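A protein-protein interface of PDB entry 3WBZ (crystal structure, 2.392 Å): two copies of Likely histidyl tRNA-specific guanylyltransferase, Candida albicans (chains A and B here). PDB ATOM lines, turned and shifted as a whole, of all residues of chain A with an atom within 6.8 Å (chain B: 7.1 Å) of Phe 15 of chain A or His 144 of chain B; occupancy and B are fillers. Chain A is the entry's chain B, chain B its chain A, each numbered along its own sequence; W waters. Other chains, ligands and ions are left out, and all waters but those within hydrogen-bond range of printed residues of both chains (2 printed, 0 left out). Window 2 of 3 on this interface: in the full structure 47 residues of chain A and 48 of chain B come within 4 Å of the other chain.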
ATOM      1  N   TYR A   9     -26.088 -19.740 -32.669  1.00  0.00           N
ATOM      2  CA  TYR A   9     -25.112 -18.728 -32.285  1.00  0.00           C
ATOM      3  C   TYR A   9     -25.735 -17.528 -31.549  1.00  0.00           C
ATOM      4  O   TYR A   9     -25.007 -16.746 -30.921  1.00  0.00           O
ATOM      5  CB  TYR A   9     -24.334 -18.214 -33.512  1.00  0.00           C
ATOM      6  CG  TYR A   9     -23.678 -19.297 -34.345  1.00  0.00           C
ATOM      7  CD1 TYR A   9     -22.712 -20.132 -33.800  1.00  0.00           C
ATOM      8  CD2 TYR A   9     -24.002 -19.458 -35.691  1.00  0.00           C
ATOM      9  CE1 TYR A   9     -22.120 -21.130 -34.561  1.00  0.00           C
ATOM     10  CE2 TYR A   9     -23.413 -20.445 -36.456  1.00  0.00           C
ATOM     11  CZ  TYR A   9     -22.472 -21.280 -35.884  1.00  0.00           C
ATOM     12  OH  TYR A   9     -21.870 -22.253 -36.643  1.00  0.00           O
ATOM     13  N   TYR A  11     -27.392 -17.120 -28.829  1.00  0.00           N
ATOM     14  CA  TYR A  11     -27.319 -17.103 -27.361  1.00  0.00           C
ATOM     15  C   TYR A  11     -26.306 -16.027 -26.891  1.00  0.00           C
ATOM     16  O   TYR A  11     -26.427 -15.508 -25.779  1.00  0.00           O
ATOM     17  CB  TYR A  11     -26.932 -18.507 -26.795  1.00  0.00           C
ATOM     18  CG  TYR A  11     -25.443 -18.771 -26.899  1.00  0.00           C
ATOM     19  CD1 TYR A  11     -24.886 -19.275 -28.079  1.00  0.00           C
ATOM     20  CD2 TYR A  11     -24.582 -18.442 -25.848  1.00  0.00           C
ATOM     21  CE1 TYR A  11     -23.518 -19.463 -28.193  1.00  0.00           C
ATOM     22  CE2 TYR A  11     -23.224 -18.619 -25.951  1.00  0.00           C
ATOM     23  CZ  TYR A  11     -22.687 -19.125 -27.122  1.00  0.00           C
ATOM     24  OH  TYR A  11     -21.321 -19.307 -27.212  1.00  0.00           O
ATOM     25  N   VAL A  12     -25.331 -15.680 -27.735  1.00  0.00           N
ATOM     26  CA  VAL A  12     -24.293 -14.711 -27.367  1.00  0.00           C
ATOM     27  C   VAL A  12     -24.893 -13.339 -27.061  1.00  0.00           C
ATOM     28  O   VAL A  12     -24.272 -12.496 -26.399  1.00  0.00           O
ATOM     29  CB  VAL A  12     -23.216 -14.541 -28.482  1.00  0.00           C
ATOM     30  CG1 VAL A  12     -22.450 -15.827 -28.728  1.00  0.00           C
ATOM     31  CG2 VAL A  12     -23.827 -13.986 -29.780  1.00  0.00           C
ATOM     32  N   LYS A  13     -26.114 -13.129 -27.542  1.00  0.00           N
ATOM     33  CA  LYS A  13     -26.858 -11.902 -27.283  1.00  0.00           C
ATOM     34  C   LYS A  13     -27.173 -11.780 -25.800  1.00  0.00           C
ATOM     35  O   LYS A  13     -27.316 -10.682 -25.285  1.00  0.00           O
ATOM     36  CB  LYS A  13     -28.143 -11.889 -28.125  1.00  0.00           C
ATOM     37  CG  LYS A  13     -29.012 -10.674 -27.959  1.00  0.00           C
ATOM     38  CD  LYS A  13     -28.444  -9.459 -28.629  1.00  0.00           C
ATOM     39  CE  LYS A  13     -29.541  -8.448 -28.888  1.00  0.00           C
ATOM     40  NZ  LYS A  13     -29.063  -7.062 -28.688  1.00  0.00           N
ATOM     41  N   LEU A  14     -27.242 -12.909 -25.107  1.00  0.00           N
ATOM     42  CA  LEU A  14     -27.610 -12.925 -23.686  1.00  0.00           C
ATOM     43  C   LEU A  14     -26.515 -12.371 -22.774  1.00  0.00           C
ATOM     44  O   LEU A  14     -26.745 -12.214 -21.579  1.00  0.00           O
ATOM     45  CB  LEU A  14     -27.960 -14.349 -23.231  1.00  0.00           C
ATOM     46  CG  LEU A  14     -29.146 -15.026 -23.933  1.00  0.00           C
ATOM     47  CD1 LEU A  14     -29.259 -16.496 -23.545  1.00  0.00           C
ATOM     48  CD2 LEU A  14     -30.456 -14.288 -23.636  1.00  0.00           C
ATOM     49  N   PHE A  15     -25.331 -12.095 -23.328  1.00  0.00           N
ATOM     50  CA  PHE A  15     -24.219 -11.553 -22.543  1.00  0.00           C
ATOM     51  C   PHE A  15     -24.292 -10.026 -22.443  1.00  0.00           C
ATOM     52  O   PHE A  15     -23.547  -9.416 -21.672  1.00  0.00           O
ATOM     53  CB  PHE A  15     -22.859 -11.991 -23.138  1.00  0.00           C
ATOM     54  CG  PHE A  15     -22.522 -13.463 -22.912  1.00  0.00           C
ATOM     55  CD1 PHE A  15     -23.216 -14.465 -23.576  1.00  0.00           C
ATOM     56  CD2 PHE A  15     -21.504 -13.833 -22.043  1.00  0.00           C
ATOM     57  CE1 PHE A  15     -22.910 -15.816 -23.364  1.00  0.00           C
ATOM     58  CE2 PHE A  15     -21.180 -15.175 -21.839  1.00  0.00           C
ATOM     59  CZ  PHE A  15     -21.888 -16.171 -22.505  1.00  0.00           C
ATOM     60  N   GLU A  16     -25.190  -9.405 -23.219  1.00  0.00           N
ATOM     61  CA  GLU A  16     -25.351  -7.940 -23.197  1.00  0.00           C
ATOM     62  C   GLU A  16     -26.024  -7.560 -21.898  1.00  0.00           C
ATOM     63  O   GLU A  16     -26.856  -8.292 -21.397  1.00  0.00           O
ATOM     64  CB  GLU A  16     -26.184  -7.441 -24.380  1.00  0.00           C
ATOM     65  CG  GLU A  16     -25.572  -7.806 -25.713  1.00  0.00           C
ATOM     66  CD  GLU A  16     -26.255  -7.178 -26.929  1.00  0.00           C
ATOM     67  OE1 GLU A  16     -27.036  -6.204 -26.779  1.00  0.00           O
ATOM     68  OE2 GLU A  16     -26.003  -7.694 -28.046  1.00  0.00           O
ATOM     69  N   LYS A  17     -25.633  -6.434 -21.332  1.00  0.00           N
ATOM     70  CA  LYS A  17     -26.216  -5.946 -20.098  1.00  0.00           C
ATOM     71  C   LYS A  17     -26.639  -4.505 -20.330  1.00  0.00           C
ATOM     72  O   LYS A  17     -25.804  -3.687 -20.673  1.00  0.00           O
ATOM     73  CB  LYS A  17     -25.220  -6.065 -18.940  1.00  0.00           C
ATOM     74  CG  LYS A  17     -25.750  -5.500 -17.649  1.00  0.00           C
ATOM     75  CD  LYS A  17     -24.849  -5.823 -16.463  1.00  0.00           C
ATOM     76  CE  LYS A  17     -25.126  -7.280 -16.045  1.00  0.00           C
ATOM     77  NZ  LYS A  17     -24.397  -7.720 -14.819  1.00  0.00           N
ATOM     78  N   ILE B  28     -16.244  -7.115 -26.889  1.00  0.00           N
ATOM     79  CA  ILE B  28     -16.754  -6.797 -28.213  1.00  0.00           C
ATOM     80  C   ILE B  28     -17.444  -5.440 -28.173  1.00  0.00           C
ATOM     81  O   ILE B  28     -18.296  -5.198 -27.330  1.00  0.00           O
ATOM     82  CB  ILE B  28     -17.754  -7.874 -28.712  1.00  0.00           C
ATOM     83  CG1 ILE B  28     -17.016  -9.178 -29.050  1.00  0.00           C
ATOM     84  CG2 ILE B  28     -18.567  -7.369 -29.920  1.00  0.00           C
ATOM     85  CD1 ILE B  28     -16.290  -9.160 -30.364  1.00  0.00           C
ATOM     86  N   ALA B 136     -20.784  -2.209 -25.543  1.00  0.00           N
ATOM     87  CA  ALA B 136     -19.721  -3.124 -25.185  1.00  0.00           C
ATOM     88  C   ALA B 136     -20.355  -4.383 -24.586  1.00  0.00           C
ATOM     89  O   ALA B 136     -21.279  -4.282 -23.784  1.00  0.00           O
ATOM     90  CB  ALA B 136     -18.760  -2.460 -24.201  1.00  0.00           C
ATOM     91  N   VAL B 137     -19.889  -5.554 -25.003  1.00  0.00           N
ATOM     92  CA  VAL B 137     -20.348  -6.807 -24.442  1.00  0.00           C
ATOM     93  C   VAL B 137     -19.111  -7.624 -24.028  1.00  0.00           C
ATOM     94  O   VAL B 137     -18.122  -7.666 -24.748  1.00  0.00           O
ATOM     95  CB  VAL B 137     -21.235  -7.611 -25.455  1.00  0.00           C
ATOM     96  CG1 VAL B 137     -21.972  -8.722 -24.753  1.00  0.00           C
ATOM     97  CG2 VAL B 137     -22.243  -6.692 -26.177  1.00  0.00           C
ATOM     98  N   LEU B 138     -19.167  -8.236 -22.850  1.00  0.00           N
ATOM     99  CA  LEU B 138     -18.074  -9.054 -22.329  1.00  0.00           C
ATOM    100  C   LEU B 138     -18.296 -10.524 -22.630  1.00  0.00           C
ATOM    101  O   LEU B 138     -19.389 -11.057 -22.394  1.00  0.00           O
ATOM    102  CB  LEU B 138     -17.936  -8.870 -20.810  1.00  0.00           C
ATOM    103  CG  LEU B 138     -17.619  -7.464 -20.304  1.00  0.00           C
ATOM    104  CD1 LEU B 138     -17.675  -7.350 -18.789  1.00  0.00           C
ATOM    105  CD2 LEU B 138     -16.242  -7.086 -20.802  1.00  0.00           C
ATOM    106  N   TYR B 139     -17.249 -11.200 -23.087  1.00  0.00           N
ATOM    107  CA  TYR B 139     -17.320 -12.648 -23.306  1.00  0.00           C
ATOM    108  C   TYR B 139     -16.136 -13.287 -22.584  1.00  0.00           C
ATOM    109  O   TYR B 139     -14.990 -12.923 -22.830  1.00  0.00           O
ATOM    110  CB  TYR B 139     -17.319 -12.975 -24.805  1.00  0.00           C
ATOM    111  CG  TYR B 139     -18.575 -12.501 -25.537  1.00  0.00           C
ATOM    112  CD1 TYR B 139     -19.758 -13.205 -25.423  1.00  0.00           C
ATOM    113  CD2 TYR B 139     -18.580 -11.328 -26.308  1.00  0.00           C
ATOM    114  CE1 TYR B 139     -20.904 -12.797 -26.062  1.00  0.00           C
ATOM    115  CE2 TYR B 139     -19.740 -10.905 -26.965  1.00  0.00           C
ATOM    116  CZ  TYR B 139     -20.909 -11.651 -26.824  1.00  0.00           C
ATOM    117  OH  TYR B 139     -22.097 -11.274 -27.446  1.00  0.00           O
ATOM    118  N   PRO B 140     -16.414 -14.211 -21.648  1.00  0.00           N
ATOM    119  CA  PRO B 140     -15.390 -14.769 -20.754  1.00  0.00           C
ATOM    120  C   PRO B 140     -14.550 -15.884 -21.372  1.00  0.00           C
ATOM    121  O   PRO B 140     -13.614 -16.336 -20.718  1.00  0.00           O
ATOM    122  CB  PRO B 140     -16.211 -15.332 -19.598  1.00  0.00           C
ATOM    123  CG  PRO B 140     -17.468 -15.772 -20.246  1.00  0.00           C
ATOM    124  CD  PRO B 140     -17.752 -14.721 -21.320  1.00  0.00           C
ATOM    125  N   ASP B 141     -14.915 -16.355 -22.562  1.00  0.00           N
ATOM    126  CA  ASP B 141     -14.224 -17.480 -23.191  1.00  0.00           C
ATOM    127  C   ASP B 141     -14.160 -17.279 -24.691  1.00  0.00           C
ATOM    128  O   ASP B 141     -15.122 -16.774 -25.287  1.00  0.00           O
ATOM    129  CB  ASP B 141     -14.942 -18.799 -22.875  1.00  0.00           C
ATOM    130  CG  ASP B 141     -14.100 -20.026 -23.191  1.00  0.00           C
ATOM    131  OD1 ASP B 141     -13.842 -20.336 -24.381  1.00  0.00           O
ATOM    132  OD2 ASP B 141     -13.718 -20.703 -22.224  1.00  0.00           O
ATOM    133  N   PHE B 142     -13.048 -17.672 -25.313  1.00  0.00           N
ATOM    134  CA  PHE B 142     -12.884 -17.428 -26.744  1.00  0.00           C
ATOM    135  C   PHE B 142     -13.903 -18.196 -27.603  1.00  0.00           C
ATOM    136  O   PHE B 142     -14.163 -17.814 -28.730  1.00  0.00           O
ATOM    137  CB  PHE B 142     -11.462 -17.737 -27.209  1.00  0.00           C
ATOM    138  CG  PHE B 142     -11.146 -17.166 -28.579  1.00  0.00           C
ATOM    139  CD1 PHE B 142     -10.876 -15.807 -28.731  1.00  0.00           C
ATOM    140  CD2 PHE B 142     -11.121 -17.979 -29.710  1.00  0.00           C
ATOM    141  CE1 PHE B 142     -10.583 -15.282 -29.972  1.00  0.00           C
ATOM    142  CE2 PHE B 142     -10.826 -17.449 -30.958  1.00  0.00           C
ATOM    143  CZ  PHE B 142     -10.562 -16.102 -31.086  1.00  0.00           C
ATOM    144  N   LYS B 143     -14.470 -19.283 -27.087  1.00  0.00           N
ATOM    145  CA  LYS B 143     -15.503 -19.984 -27.851  1.00  0.00           C
ATOM    146  C   LYS B 143     -16.744 -19.086 -28.073  1.00  0.00           C
ATOM    147  O   LYS B 143     -17.455 -19.230 -29.063  1.00  0.00           O
ATOM    148  CB  LYS B 143     -15.889 -21.291 -27.151  1.00  0.00           C
ATOM    149  CG  LYS B 143     -16.809 -21.130 -25.958  1.00  0.00           C
ATOM    150  CD  LYS B 143     -16.862 -22.399 -25.109  1.00  0.00           C
ATOM    151  CE  LYS B 143     -17.830 -22.209 -23.936  1.00  0.00           C
ATOM    152  NZ  LYS B 143     -17.794 -23.304 -22.911  1.00  0.00           N
ATOM    153  N   HIS B 144     -16.987 -18.133 -27.177  1.00  0.00           N
ATOM    154  CA  HIS B 144     -18.132 -17.242 -27.361  1.00  0.00           C
ATOM    155  C   HIS B 144     -17.813 -16.195 -28.423  1.00  0.00           C
ATOM    156  O   HIS B 144     -18.690 -15.741 -29.147  1.00  0.00           O
ATOM    157  CB  HIS B 144     -18.525 -16.572 -26.040  1.00  0.00           C
ATOM    158  CG  HIS B 144     -18.900 -17.548 -24.964  1.00  0.00           C
ATOM    159  ND1 HIS B 144     -19.870 -18.504 -25.138  1.00  0.00           N
ATOM    160  CD2 HIS B 144     -18.422 -17.711 -23.706  1.00  0.00           C
ATOM    161  CE1 HIS B 144     -19.977 -19.225 -24.032  1.00  0.00           C
ATOM    162  NE2 HIS B 144     -19.111 -18.763 -23.152  1.00  0.00           N
ATOM    163  N   ILE B 145     -16.528 -15.884 -28.546  1.00  0.00           N
ATOM    164  CA  ILE B 145     -16.029 -14.973 -29.555  1.00  0.00           C
ATOM    165  C   ILE B 145     -16.187 -15.580 -30.954  1.00  0.00           C
ATOM    166  O   ILE B 145     -16.654 -14.914 -31.875  1.00  0.00           O
ATOM    167  CB  ILE B 145     -14.539 -14.624 -29.292  1.00  0.00           C
ATOM    168  CG1 ILE B 145     -14.389 -13.940 -27.937  1.00  0.00           C
ATOM    169  CG2 ILE B 145     -13.958 -13.775 -30.429  1.00  0.00           C
ATOM    170  CD1 ILE B 145     -15.213 -12.710 -27.802  1.00  0.00           C
ATOM    171  N   ARG B 146     -15.801 -16.839 -31.111  1.00  0.00           N
ATOM    172  CA  ARG B 146     -16.038 -17.547 -32.365  1.00  0.00           C
ATOM    173  C   ARG B 146     -17.525 -17.527 -32.712  1.00  0.00           C
ATOM    174  O   ARG B 146     -17.916 -17.276 -33.852  1.00  0.00           O
ATOM    175  CB  ARG B 146     -15.578 -19.008 -32.283  1.00  0.00           C
ATOM    176  CG  ARG B 146     -14.096 -19.246 -32.247  1.00  0.00           C
ATOM    177  CD  ARG B 146     -13.529 -18.991 -33.613  1.00  0.00           C
ATOM    178  NE  ARG B 146     -14.298 -19.634 -34.681  1.00  0.00           N
ATOM    179  CZ  ARG B 146     -14.125 -20.882 -35.102  1.00  0.00           C
ATOM    180  NH1 ARG B 146     -13.193 -21.652 -34.553  1.00  0.00           N
ATOM    181  NH2 ARG B 146     -14.880 -21.353 -36.088  1.00  0.00           N
ATOM    182  N   ASN B 147     -18.355 -17.851 -31.730  1.00  0.00           N
ATOM    183  CA  ASN B 147     -19.789 -17.902 -31.965  1.00  0.00           C
ATOM    184  C   ASN B 147     -20.402 -16.530 -32.249  1.00  0.00           C
ATOM    185  O   ASN B 147     -21.371 -16.425 -33.001  1.00  0.00           O
ATOM    186  CB  ASN B 147     -20.488 -18.553 -30.770  1.00  0.00           C
ATOM    187  CG  ASN B 147     -20.192 -20.044 -30.670  1.00  0.00           C
ATOM    188  OD1 ASN B 147     -19.764 -20.654 -31.644  1.00  0.00           O
ATOM    189  ND2 ASN B 147     -20.408 -20.627 -29.492  1.00  0.00           N
ATOM    190  N   TYR B 148     -19.816 -15.490 -31.664  1.00  0.00           N
ATOM    191  CA  TYR B 148     -20.298 -14.145 -31.866  1.00  0.00           C
ATOM    192  C   TYR B 148     -20.109 -13.728 -33.314  1.00  0.00           C
ATOM    193  O   TYR B 148     -21.016 -13.171 -33.944  1.00  0.00           O
ATOM    194  CB  TYR B 148     -19.605 -13.145 -30.921  1.00  0.00           C
ATOM    195  CG  TYR B 148     -20.026 -11.739 -31.240  1.00  0.00           C
ATOM    196  CD1 TYR B 148     -21.173 -11.197 -30.680  1.00  0.00           C
ATOM    197  CD2 TYR B 148     -19.314 -10.971 -32.173  1.00  0.00           C
ATOM    198  CE1 TYR B 148     -21.589  -9.937 -31.014  1.00  0.00           C
ATOM    199  CE2 TYR B 148     -19.739  -9.715 -32.531  1.00  0.00           C
ATOM    200  CZ  TYR B 148     -20.859  -9.198 -31.937  1.00  0.00           C
ATOM    201  OH  TYR B 148     -21.269  -7.932 -32.265  1.00  0.00           O
ATOM    202  N   PHE B 149     -18.920 -13.951 -33.846  1.00  0.00           N
ATOM    203  CA  PHE B 149     -18.683 -13.540 -35.219  1.00  0.00           C
ATOM    204  C   PHE B 149     -19.454 -14.423 -36.181  1.00  0.00           C
ATOM    205  O   PHE B 149     -19.911 -13.959 -37.229  1.00  0.00           O
ATOM    206  CB  PHE B 149     -17.183 -13.539 -35.534  1.00  0.00           C
ATOM    207  CG  PHE B 149     -16.471 -12.376 -34.931  1.00  0.00           C
ATOM    208  CD1 PHE B 149     -16.615 -11.114 -35.479  1.00  0.00           C
ATOM    209  CD2 PHE B 149     -15.692 -12.527 -33.795  1.00  0.00           C
ATOM    210  CE1 PHE B 149     -15.973 -10.010 -34.903  1.00  0.00           C
ATOM    211  CE2 PHE B 149     -15.042 -11.444 -33.222  1.00  0.00           C
ATOM    212  CZ  PHE B 149     -15.188 -10.175 -33.776  1.00  0.00           C
ATOM    213  N   SER B 150     -19.612 -15.689 -35.814  1.00  0.00           N
ATOM    214  CA  SER B 150     -20.471 -16.602 -36.558  1.00  0.00           C
ATOM    215  C   SER B 150     -21.897 -16.097 -36.587  1.00  0.00           C
ATOM    216  O   SER B 150     -22.568 -16.194 -37.600  1.00  0.00           O
ATOM    217  CB  SER B 150     -20.410 -17.997 -35.962  1.00  0.00           C
ATOM    218  OG  SER B 150     -19.130 -18.525 -36.180  1.00  0.00           O
HETATM  219  O   HOH W   1     -23.981  -9.236 -28.432  1.00  0.00           O
HETATM  220  O   HOH W   2     -21.491  -7.711 -21.117  1.00  0.00           O
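Hydrophobic or aromatic side chains of chain A that line the printed part of chain B: Tyr 9, Tyr 11, Val 12 and Phe 15. Along chain A the printed residues that touch a printed residue of chain B span positions 9 to 16. Hydrophobic or aromatic side chains of chain B within 4 Å of the printed part of chain A: Val 137, Tyr 139, Pro 140, His 144 and Tyr 148. Along chain B the printed residues that touch a printed residue of chain A span positions 137 to 150.
Of the printed residues of chain B, Val 12 of chain A touches Tyr 139 (2.7 Å), His 144 (3.8 Å), Asn 147 (3.9 Å) and Tyr 148 (3.95 Å). Phe 15 of chain A touches five residues of chain B. Of the printed residues of chain B, Glu 16 of chain A touches Val 137 (3.5 Å). Lys 17 of chain A touches none of the printed residues of chain B. Of the printed residues of chain A, Val 137 of chain B touches Phe 15 and Glu 16. Of the printed residues of chain A, Leu 138 of chain B touches Phe 15. His 144 of chain B touches just these residues of chain A: Tyr 11 (2.7 Å), Val 12 (3.8 Å) and Phe 15 (3.9 Å). Printed residues of chain A within 4 Å of Ser 150 of chain B: Tyr 9 (3.8 Å).
Water W1 bridges the side-chain carboxylate of Glu 16 of chain A (2.6 Å) and the side-chain hydroxyl of Tyr 139 of chain B (2.9 Å). Water W2 lies within hydrogen-bond range of the backbone carbonyl oxygen of Phe 15 of chain A (2.7 Å) and the backbone NH of Leu 138 of chain B (2.9 Å).
No position is printed for both chains.
Among the printed residues, merely in contact across the chains: Phe 15 of chain A with Pro 140 of chain B (3.5 Å), Tyr 9 of chain A with Asn 147 of chain B (3.5 Å), Phe 15 of chain A with Leu 138 of chain B (3.5 Å), Phe 15 of chain A with Val 137 of chain B (3.5 Å), Glu 16 of chain A with Val 137 of chain B (3.5 Å), Phe 15 of chain A with Tyr 139 of chain B (3.6 Å), Val 12 of chain A with His 144 of chain B (3.8 Å), Tyr 9 of chain A with Ser 150 of chain B (3.8 Å), Phe 15 of chain A with His 144 of chain B (3.9 Å), Val 12 of chain A with Asn 147 of chain B (3.9 Å) and Val 12 of chain A with Tyr 148 of chain B (3.95 Å).
The side-chain hydroxyl of Tyr 139 of chain B lies within hydrogen-bond range of the backbone carbonyl oxygen of Val 12 of chain A (2.7 Å). The side-chain hydroxyl (OH) of Tyr 11 of chain A lies within hydrogen-bond range of a ring nitrogen (ND1) of His 144 of chain B. The side-chain amide nitrogen (ND2) of Asn 147 of chain B sits at hydrogen-bond distance from the side-chain hydroxyl (OH) of Tyr 11 of chain A, 2.8 Å away.
N of Val 137 of chain B is in hydrogen-bond range of O of Ile 28 of chain B (2.8 Å). O of Lys 143 of chain B lies close to ND2 of Asn 147 of chain B (3.3 Å). The backbone carbonyl oxygen (O) of Arg 146 of chain B lies within hydrogen-bond range of the side-chain hydroxyl (OG) of Ser 150 of chain B (2.9 Å). The side-chain amino group (NZ) of Lys 13 of chain A is in salt-bridge range of the side-chain carboxylate (OE1) of Glu 16 of chain A, 2.9 Å away.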
